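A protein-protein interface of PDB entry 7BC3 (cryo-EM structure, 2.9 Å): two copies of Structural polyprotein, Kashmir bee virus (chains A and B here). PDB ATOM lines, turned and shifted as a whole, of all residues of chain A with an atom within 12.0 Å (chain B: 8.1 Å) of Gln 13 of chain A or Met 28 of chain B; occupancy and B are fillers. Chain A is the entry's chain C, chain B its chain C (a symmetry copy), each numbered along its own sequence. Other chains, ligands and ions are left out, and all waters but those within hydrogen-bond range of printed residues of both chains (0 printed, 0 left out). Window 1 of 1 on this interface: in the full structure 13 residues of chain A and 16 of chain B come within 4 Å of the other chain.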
ATOM      1  N   VAL A   9     -21.364  -4.713 -19.485  1.00  0.00           N
ATOM      2  CA  VAL A   9     -21.500  -4.063 -18.187  1.00  0.00           C
ATOM      3  C   VAL A   9     -21.182  -2.582 -18.367  1.00  0.00           C
ATOM      4  O   VAL A   9     -20.041  -2.214 -18.653  1.00  0.00           O
ATOM      5  CB  VAL A   9     -20.582  -4.706 -17.143  1.00  0.00           C
ATOM      6  CG1 VAL A   9     -20.705  -3.993 -15.820  1.00  0.00           C
ATOM      7  CG2 VAL A   9     -20.909  -6.182 -16.987  1.00  0.00           C
ATOM      8  N   MET A  10     -22.186  -1.732 -18.200  1.00  0.00           N
ATOM      9  CA  MET A  10     -21.969  -0.297 -18.324  1.00  0.00           C
ATOM     10  C   MET A  10     -21.118   0.199 -17.161  1.00  0.00           C
ATOM     11  O   MET A  10     -21.394  -0.149 -16.007  1.00  0.00           O
ATOM     12  CB  MET A  10     -23.300   0.454 -18.338  1.00  0.00           C
ATOM     13  CG  MET A  10     -24.221   0.102 -19.491  1.00  0.00           C
ATOM     14  SD  MET A  10     -23.591   0.629 -21.089  1.00  0.00           S
ATOM     15  CE  MET A  10     -23.298  -0.936 -21.860  1.00  0.00           C
ATOM     16  N   PRO A  11     -20.089   1.010 -17.412  1.00  0.00           N
ATOM     17  CA  PRO A  11     -19.446   1.735 -16.313  1.00  0.00           C
ATOM     18  C   PRO A  11     -20.168   3.051 -16.078  1.00  0.00           C
ATOM     19  O   PRO A  11     -20.590   3.718 -17.026  1.00  0.00           O
ATOM     20  CB  PRO A  11     -18.022   1.958 -16.822  1.00  0.00           C
ATOM     21  CG  PRO A  11     -18.191   2.077 -18.295  1.00  0.00           C
ATOM     22  CD  PRO A  11     -19.386   1.237 -18.688  1.00  0.00           C
ATOM     23  N   LEU A  12     -20.315   3.427 -14.813  1.00  0.00           N
ATOM     24  CA  LEU A  12     -21.102   4.593 -14.461  1.00  0.00           C
ATOM     25  C   LEU A  12     -20.425   5.412 -13.377  1.00  0.00           C
ATOM     26  O   LEU A  12     -19.378   5.039 -12.841  1.00  0.00           O
ATOM     27  CB  LEU A  12     -22.485   4.199 -13.981  1.00  0.00           C
ATOM     28  CG  LEU A  12     -22.502   3.342 -12.716  1.00  0.00           C
ATOM     29  CD1 LEU A  12     -22.434   4.156 -11.433  1.00  0.00           C
ATOM     30  CD2 LEU A  12     -23.735   2.504 -12.728  1.00  0.00           C
ATOM     31  N   GLN A  13     -21.059   6.537 -13.058  1.00  0.00           N
ATOM     32  CA  GLN A  13     -20.606   7.455 -12.026  1.00  0.00           C
ATOM     33  C   GLN A  13     -21.834   8.103 -11.410  1.00  0.00           C
ATOM     34  O   GLN A  13     -22.621   8.737 -12.119  1.00  0.00           O
ATOM     35  CB  GLN A  13     -19.671   8.513 -12.612  1.00  0.00           C
ATOM     36  CG  GLN A  13     -18.826   9.235 -11.598  1.00  0.00           C
ATOM     37  CD  GLN A  13     -18.022  10.355 -12.216  1.00  0.00           C
ATOM     38  OE1 GLN A  13     -18.322  10.816 -13.316  1.00  0.00           O
ATOM     39  NE2 GLN A  13     -16.988  10.794 -11.515  1.00  0.00           N
ATOM     40  N   ASN A  14     -22.007   7.938 -10.099  1.00  0.00           N
ATOM     41  CA  ASN A  14     -23.145   8.527  -9.399  1.00  0.00           C
ATOM     42  C   ASN A  14     -22.813   9.985  -9.103  1.00  0.00           C
ATOM     43  O   ASN A  14     -22.422  10.364  -7.997  1.00  0.00           O
ATOM     44  CB  ASN A  14     -23.469   7.752  -8.129  1.00  0.00           C
ATOM     45  CG  ASN A  14     -24.912   7.908  -7.707  1.00  0.00           C
ATOM     46  OD1 ASN A  14     -25.595   8.843  -8.120  1.00  0.00           O
ATOM     47  ND2 ASN A  14     -25.386   6.990  -6.878  1.00  0.00           N
ATOM     48  N   VAL A  15     -22.983  10.818 -10.124  1.00  0.00           N
ATOM     49  CA  VAL A  15     -22.672  12.240 -10.027  1.00  0.00           C
ATOM     50  C   VAL A  15     -23.937  13.039 -10.320  1.00  0.00           C
ATOM     51  O   VAL A  15     -24.122  13.526 -11.445  1.00  0.00           O
ATOM     52  CB  VAL A  15     -21.518  12.622 -10.969  1.00  0.00           C
ATOM     53  CG1 VAL A  15     -21.847  12.284 -12.420  1.00  0.00           C
ATOM     54  CG2 VAL A  15     -21.162  14.093 -10.812  1.00  0.00           C
ATOM     55  N   PRO A  16     -24.833  13.197  -9.350  1.00  0.00           N
ATOM     56  CA  PRO A  16     -26.015  14.031  -9.573  1.00  0.00           C
ATOM     57  C   PRO A  16     -25.636  15.498  -9.689  1.00  0.00           C
ATOM     58  O   PRO A  16     -24.661  15.963  -9.095  1.00  0.00           O
ATOM     59  CB  PRO A  16     -26.879  13.778  -8.332  1.00  0.00           C
ATOM     60  CG  PRO A  16     -26.221  12.673  -7.580  1.00  0.00           C
ATOM     61  CD  PRO A  16     -24.798  12.645  -7.988  1.00  0.00           C
ATOM     62  N   GLY A  17     -26.427  16.227 -10.467  1.00  0.00           N
ATOM     63  CA  GLY A  17     -26.151  17.628 -10.697  1.00  0.00           C
ATOM     64  C   GLY A  17     -24.868  17.822 -11.476  1.00  0.00           C
ATOM     65  O   GLY A  17     -23.952  18.514 -11.022  1.00  0.00           O
ATOM     66  N   TRP A  18     -24.792  17.203 -12.649  1.00  0.00           N
ATOM     67  CA  TRP A  18     -23.621  17.302 -13.512  1.00  0.00           C
ATOM     68  C   TRP A  18     -23.854  18.428 -14.510  1.00  0.00           C
ATOM     69  O   TRP A  18     -24.726  18.328 -15.379  1.00  0.00           O
ATOM     70  CB  TRP A  18     -23.366  15.976 -14.224  1.00  0.00           C
ATOM     71  CG  TRP A  18     -22.034  15.894 -14.902  1.00  0.00           C
ATOM     72  CD1 TRP A  18     -20.931  15.232 -14.457  1.00  0.00           C
ATOM     73  CD2 TRP A  18     -21.665  16.491 -16.150  1.00  0.00           C
ATOM     74  NE1 TRP A  18     -19.898  15.378 -15.346  1.00  0.00           N
ATOM     75  CE2 TRP A  18     -20.323  16.148 -16.395  1.00  0.00           C
ATOM     76  CE3 TRP A  18     -22.339  17.282 -17.084  1.00  0.00           C
ATOM     77  CZ2 TRP A  18     -19.642  16.570 -17.533  1.00  0.00           C
ATOM     78  CZ3 TRP A  18     -21.662  17.699 -18.211  1.00  0.00           C
ATOM     79  CH2 TRP A  18     -20.327  17.342 -18.426  1.00  0.00           C
ATOM     80  N   GLY A  19     -23.080  19.500 -14.382  1.00  0.00           N
ATOM     81  CA  GLY A  19     -23.213  20.621 -15.287  1.00  0.00           C
ATOM     82  C   GLY A  19     -24.403  21.505 -15.010  1.00  0.00           C
ATOM     83  O   GLY A  19     -24.951  22.103 -15.941  1.00  0.00           O
ATOM     84  N   TYR A  20     -24.828  21.604 -13.749  1.00  0.00           N
ATOM     85  CA  TYR A  20     -25.949  22.471 -13.416  1.00  0.00           C
ATOM     86  C   TYR A  20     -25.583  23.943 -13.521  1.00  0.00           C
ATOM     87  O   TYR A  20     -26.479  24.786 -13.635  1.00  0.00           O
ATOM     88  CB  TYR A  20     -26.460  22.149 -12.011  1.00  0.00           C
ATOM     89  CG  TYR A  20     -25.485  22.450 -10.897  1.00  0.00           C
ATOM     90  CD1 TYR A  20     -24.573  21.499 -10.473  1.00  0.00           C
ATOM     91  CD2 TYR A  20     -25.490  23.680 -10.258  1.00  0.00           C
ATOM     92  CE1 TYR A  20     -23.686  21.766  -9.453  1.00  0.00           C
ATOM     93  CE2 TYR A  20     -24.608  23.957  -9.237  1.00  0.00           C
ATOM     94  CZ  TYR A  20     -23.708  22.996  -8.838  1.00  0.00           C
ATOM     95  OH  TYR A  20     -22.827  23.267  -7.818  1.00  0.00           O
ATOM     96  N   LEU A  22     -23.883  25.202 -16.034  1.00  0.00           N
ATOM     97  CA  LEU A  22     -23.885  25.565 -17.440  1.00  0.00           C
ATOM     98  C   LEU A  22     -25.268  26.060 -17.857  1.00  0.00           C
ATOM     99  O   LEU A  22     -26.267  25.839 -17.169  1.00  0.00           O
ATOM    100  CB  LEU A  22     -23.470  24.368 -18.294  1.00  0.00           C
ATOM    101  CG  LEU A  22     -22.274  23.551 -17.792  1.00  0.00           C
ATOM    102  CD1 LEU A  22     -22.012  22.367 -18.702  1.00  0.00           C
ATOM    103  CD2 LEU A  22     -21.031  24.405 -17.683  1.00  0.00           C
ATOM    104  N   MET A  28     -32.412  17.534 -15.280  1.00  0.00           N
ATOM    105  CA  MET A  28     -33.092  16.437 -14.616  1.00  0.00           C
ATOM    106  C   MET A  28     -34.091  16.924 -13.579  1.00  0.00           C
ATOM    107  O   MET A  28     -34.390  16.198 -12.624  1.00  0.00           O
ATOM    108  CB  MET A  28     -32.063  15.509 -13.975  1.00  0.00           C
ATOM    109  CG  MET A  28     -31.195  14.785 -14.990  1.00  0.00           C
ATOM    110  SD  MET A  28     -32.134  13.677 -16.052  1.00  0.00           S
ATOM    111  CE  MET A  28     -32.863  12.608 -14.821  1.00  0.00           C
ATOM    112  N   LEU B  12     -24.319  -3.090 -14.615  1.00  0.00           N
ATOM    113  CA  LEU B  12     -23.430  -1.950 -14.500  1.00  0.00           C
ATOM    114  C   LEU B  12     -22.286  -2.233 -13.542  1.00  0.00           C
ATOM    115  O   LEU B  12     -22.219  -3.288 -12.908  1.00  0.00           O
ATOM    116  CB  LEU B  12     -24.174  -0.719 -14.019  1.00  0.00           C
ATOM    117  CG  LEU B  12     -24.794  -0.850 -12.628  1.00  0.00           C
ATOM    118  CD1 LEU B  12     -23.823  -0.541 -11.500  1.00  0.00           C
ATOM    119  CD2 LEU B  12     -25.977   0.054 -12.550  1.00  0.00           C
ATOM    120  N   GLN B  13     -21.392  -1.253 -13.446  1.00  0.00           N
ATOM    121  CA  GLN B  13     -20.236  -1.299 -12.567  1.00  0.00           C
ATOM    122  C   GLN B  13     -19.935   0.123 -12.123  1.00  0.00           C
ATOM    123  O   GLN B  13     -19.700   0.998 -12.962  1.00  0.00           O
ATOM    124  CB  GLN B  13     -19.031  -1.909 -13.284  1.00  0.00           C
ATOM    125  CG  GLN B  13     -17.935  -2.387 -12.372  1.00  0.00           C
ATOM    126  CD  GLN B  13     -16.719  -2.858 -13.137  1.00  0.00           C
ATOM    127  OE1 GLN B  13     -16.546  -2.534 -14.310  1.00  0.00           O
ATOM    128  NE2 GLN B  13     -15.871  -3.633 -12.477  1.00  0.00           N
ATOM    129  N   ASN B  14     -19.952   0.358 -10.811  1.00  0.00           N
ATOM    130  CA  ASN B  14     -19.664   1.684 -10.269  1.00  0.00           C
ATOM    131  C   ASN B  14     -18.151   1.851 -10.211  1.00  0.00           C
ATOM    132  O   ASN B  14     -17.506   1.704  -9.170  1.00  0.00           O
ATOM    133  CB  ASN B  14     -20.306   1.868  -8.901  1.00  0.00           C
ATOM    134  CG  ASN B  14     -20.563   3.322  -8.573  1.00  0.00           C
ATOM    135  OD1 ASN B  14     -19.970   4.219  -9.168  1.00  0.00           O
ATOM    136  ND2 ASN B  14     -21.452   3.563  -7.621  1.00  0.00           N
ATOM    137  N   VAL B  15     -17.578   2.175 -11.366  1.00  0.00           N
ATOM    138  CA  VAL B  15     -16.133   2.332 -11.498  1.00  0.00           C
ATOM    139  C   VAL B  15     -15.836   3.749 -11.976  1.00  0.00           C
ATOM    140  O   VAL B  15     -15.606   3.970 -13.173  1.00  0.00           O
ATOM    141  CB  VAL B  15     -15.542   1.271 -12.442  1.00  0.00           C
ATOM    142  CG1 VAL B  15     -16.178   1.340 -13.827  1.00  0.00           C
ATOM    143  CG2 VAL B  15     -14.029   1.407 -12.522  1.00  0.00           C
ATOM    144  N   PRO B  16     -15.834   4.737 -11.086  1.00  0.00           N
ATOM    145  CA  PRO B  16     -15.468   6.093 -11.497  1.00  0.00           C
ATOM    146  C   PRO B  16     -13.991   6.180 -11.843  1.00  0.00           C
ATOM    147  O   PRO B  16     -13.155   5.459 -11.297  1.00  0.00           O
ATOM    148  CB  PRO B  16     -15.801   6.950 -10.268  1.00  0.00           C
ATOM    149  CG  PRO B  16     -16.512   6.054  -9.312  1.00  0.00           C
ATOM    150  CD  PRO B  16     -16.138   4.660  -9.649  1.00  0.00           C
ATOM    151  N   GLY B  17     -13.679   7.082 -12.767  1.00  0.00           N
ATOM    152  CA  GLY B  17     -12.314   7.235 -13.219  1.00  0.00           C
ATOM    153  C   GLY B  17     -11.834   6.010 -13.964  1.00  0.00           C
ATOM    154  O   GLY B  17     -10.824   5.401 -13.597  1.00  0.00           O
ATOM    155  N   TRP B  18     -12.561   5.634 -15.011  1.00  0.00           N
ATOM    156  CA  TRP B  18     -12.219   4.476 -15.829  1.00  0.00           C
ATOM    157  C   TRP B  18     -11.388   4.952 -17.012  1.00  0.00           C
ATOM    158  O   TRP B  18     -11.890   5.664 -17.888  1.00  0.00           O
ATOM    159  CB  TRP B  18     -13.481   3.755 -16.295  1.00  0.00           C
ATOM    160  CG  TRP B  18     -13.228   2.406 -16.891  1.00  0.00           C
ATOM    161  CD1 TRP B  18     -13.426   1.200 -16.294  1.00  0.00           C
ATOM    162  CD2 TRP B  18     -12.735   2.125 -18.206  1.00  0.00           C
ATOM    163  NE1 TRP B  18     -13.088   0.185 -17.151  1.00  0.00           N
ATOM    164  CE2 TRP B  18     -12.660   0.726 -18.332  1.00  0.00           C
ATOM    165  CE3 TRP B  18     -12.350   2.921 -19.288  1.00  0.00           C
ATOM    166  CZ2 TRP B  18     -12.213   0.106 -19.494  1.00  0.00           C
ATOM    167  CZ3 TRP B  18     -11.908   2.304 -20.440  1.00  0.00           C
ATOM    168  CH2 TRP B  18     -11.843   0.911 -20.534  1.00  0.00           C
ATOM    169  N   GLY B  25     -10.256   9.165 -24.939  1.00  0.00           N
ATOM    170  CA  GLY B  25     -11.467   8.810 -24.230  1.00  0.00           C
ATOM    171  C   GLY B  25     -12.297  10.042 -23.959  1.00  0.00           C
ATOM    172  O   GLY B  25     -11.895  11.168 -24.229  1.00  0.00           O
ATOM    173  N   ILE B  26     -13.481   9.811 -23.413  1.00  0.00           N
ATOM    174  CA  ILE B  26     -14.418  10.882 -23.108  1.00  0.00           C
ATOM    175  C   ILE B  26     -14.337  11.170 -21.618  1.00  0.00           C
ATOM    176  O   ILE B  26     -14.681  10.320 -20.789  1.00  0.00           O
ATOM    177  CB  ILE B  26     -15.845  10.515 -23.537  1.00  0.00           C
ATOM    178  CG1 ILE B  26     -15.919  10.464 -25.062  1.00  0.00           C
ATOM    179  CG2 ILE B  26     -16.829  11.525 -22.998  1.00  0.00           C
ATOM    180  CD1 ILE B  26     -17.094   9.703 -25.598  1.00  0.00           C
ATOM    181  N   ASP B  27     -13.877  12.371 -21.279  1.00  0.00           N
ATOM    182  CA  ASP B  27     -13.617  12.722 -19.894  1.00  0.00           C
ATOM    183  C   ASP B  27     -14.899  13.166 -19.209  1.00  0.00           C
ATOM    184  O   ASP B  27     -15.691  13.924 -19.777  1.00  0.00           O
ATOM    185  CB  ASP B  27     -12.570  13.829 -19.813  1.00  0.00           C
ATOM    186  CG  ASP B  27     -11.782  13.791 -18.519  1.00  0.00           C
ATOM    187  OD1 ASP B  27     -12.158  13.021 -17.611  1.00  0.00           O
ATOM    188  OD2 ASP B  27     -10.783  14.528 -18.412  1.00  0.00           O
ATOM    189  N   MET B  28     -15.094  12.695 -17.981  1.00  0.00           N
ATOM    190  CA  MET B  28     -16.243  13.060 -17.170  1.00  0.00           C
ATOM    191  C   MET B  28     -15.956  14.254 -16.273  1.00  0.00           C
ATOM    192  O   MET B  28     -16.592  14.400 -15.223  1.00  0.00           O
ATOM    193  CB  MET B  28     -16.684  11.858 -16.337  1.00  0.00           C
ATOM    194  CG  MET B  28     -17.231  10.716 -17.176  1.00  0.00           C
ATOM    195  SD  MET B  28     -18.726  11.160 -18.074  1.00  0.00           S
ATOM    196  CE  MET B  28     -19.780  11.632 -16.712  1.00  0.00           C
ATOM    197  N   SER B  29     -15.014  15.105 -16.665  1.00  0.00           N
ATOM    198  CA  SER B  29     -14.678  16.284 -15.884  1.00  0.00           C
ATOM    199  C   SER B  29     -15.708  17.378 -16.124  1.00  0.00           C
ATOM    200  O   SER B  29     -16.023  17.706 -17.271  1.00  0.00           O
ATOM    201  CB  SER B  29     -13.283  16.781 -16.256  1.00  0.00           C
ATOM    202  OG  SER B  29     -12.281  15.980 -15.656  1.00  0.00           O
ATOM    203  N   VAL B  30     -16.231  17.940 -15.044  1.00  0.00           N
ATOM    204  CA  VAL B  30     -17.253  18.981 -15.157  1.00  0.00           C
ATOM    205  C   VAL B  30     -16.565  20.320 -15.402  1.00  0.00           C
ATOM    206  O   VAL B  30     -15.679  20.704 -14.622  1.00  0.00           O
ATOM    207  CB  VAL B  30     -18.110  19.029 -13.901  1.00  0.00           C
ATOM    208  CG1 VAL B  30     -19.071  20.193 -13.971  1.00  0.00           C
ATOM    209  CG2 VAL B  30     -18.866  17.731 -13.729  1.00  0.00           C
ATOM    210  N   PRO B  31     -16.933  21.052 -16.453  1.00  0.00           N
ATOM    211  CA  PRO B  31     -16.303  22.351 -16.703  1.00  0.00           C
ATOM    212  C   PRO B  31     -16.950  23.476 -15.913  1.00  0.00           C
ATOM    213  O   PRO B  31     -18.171  23.646 -15.900  1.00  0.00           O
ATOM    214  CB  PRO B  31     -16.511  22.541 -18.210  1.00  0.00           C
ATOM    215  CG  PRO B  31     -17.767  21.824 -18.500  1.00  0.00           C
ATOM    216  CD  PRO B  31     -17.867  20.681 -17.530  1.00  0.00           C
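The backbone carbonyl oxygen of Met 10 of chain A sits at hydrogen-bond distance from the backbone NH of Gln 13 of chain B (2.8 Å). The backbone NH (N) of Leu 12 of chain A lies within hydrogen-bond range of the backbone carbonyl oxygen (O) of Gln 13 of chain B (3.1 Å). O of Met 28 of chain B sits at hydrogen-bond distance from NE1 of Trp 18 of chain A (3.4 Å).
The side-chain hydroxyl (OG) of Ser 29 of chain B lies within hydrogen-bond range of the side-chain carboxylate (OD2) of Asp 27 of chain B (3.5 Å).
Among the printed residues, merely in contact across the chains: Val 9 of chain A with Leu 12 of chain B, Val 9 of chain A with Gln 13 of chain B, Met 10 of chain A with Leu 12 of chain B, Pro 11 of chain A with Gln 13 of chain B, Pro 11 of chain A with Val 15 of chain B, Leu 12 of chain A with Leu 12 of chain B, Leu 12 of chain A with Asn 14 of chain B, Leu 12 of chain A with Val 15 of chain B, Leu 12 of chain A with Pro 16 of chain B, Gln 13 of chain A with Met 28 of chain B, Trp 18 of chain A with Ser 29 of chain B, Trp 18 of chain A with Val 30 of chain B and Leu 22 of chain A with Pro 31 of chain B.
Printed residues of chain B within 4 Å of Gln 13 of chain A: Met 28. Met 28 of chain B touches just these residues of chain A: Gln 13 (3.6 Å) and Trp 18 (3.4 Å). Of chain A, only Leu 12 comes within 4 Å of Asn 14 of chain B. No residue of chain A comes within 4 Å of Ile 26 of chain B. No residue of chain A comes within 4 Å of Asp 27 of chain B. Ser 29 of chain B touches just one residue of chain A: Trp 18. Val 30 of chain B touches one residue of chain A. Of the printed residues of chain B, Leu 12 of chain A touches Leu 12, Gln 13, Asn 14, Val 15 and Pro 16. Of the printed residues of chain B, Met 10 of chain A touches Leu 12 and Gln 13. Of the printed residues of chain B, Leu 22 of chain A touches Pro 31. The nearest residue of chain A that does not touch Met 28 of chain B is Val 15 of chain A (4.8 Å). The nearest printed residue of chain B that does not touch Leu 12 of chain A is Gly 17 of chain B (6.1 Å).
Of the 14 printed residues of chain B, 9 touch a printed residue of chain A. Hydrophobic or aromatic side chains of chain B within 4 Å of the printed part of chain A: Leu 12, Val 15, Met 28 and Val 30. Of the 14 printed residues of chain A, 7 touch a printed residue of chain B. Hydrophobic or aromatic side chains of chain A within 4 Å of the printed part of chain B: Val 9, Pro 11, Leu 12, Trp 18 and Leu 22. Among the printed residues, no Asp or Glu carboxylate lies within 4 Å of a Lys or Arg side-chain nitrogen of the other chain.
Leu 12 of chain A touches its own counterpart, Leu 12 of chain B. Leu 12 of chain A touches Gln 13 of chain B, but with the chains exchanged Gln 13 of chain A does not touch Leu 12 of chain B (7.8 Å). Leu 12 of chain A touches Val 15 of chain B, but with the chains exchanged Val 15 of chain A does not touch Leu 12 of chain B (11.4 Å). Trp 18 of chain A touches Met 28 of chain B, but with the chains exchanged Met 28 of chain A does not touch Trp 18 of chain B (20.8 Å). Of the 16 pairs that touch across the chains among the printed residues, 1 has its exchanged pair printed and touching as well.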
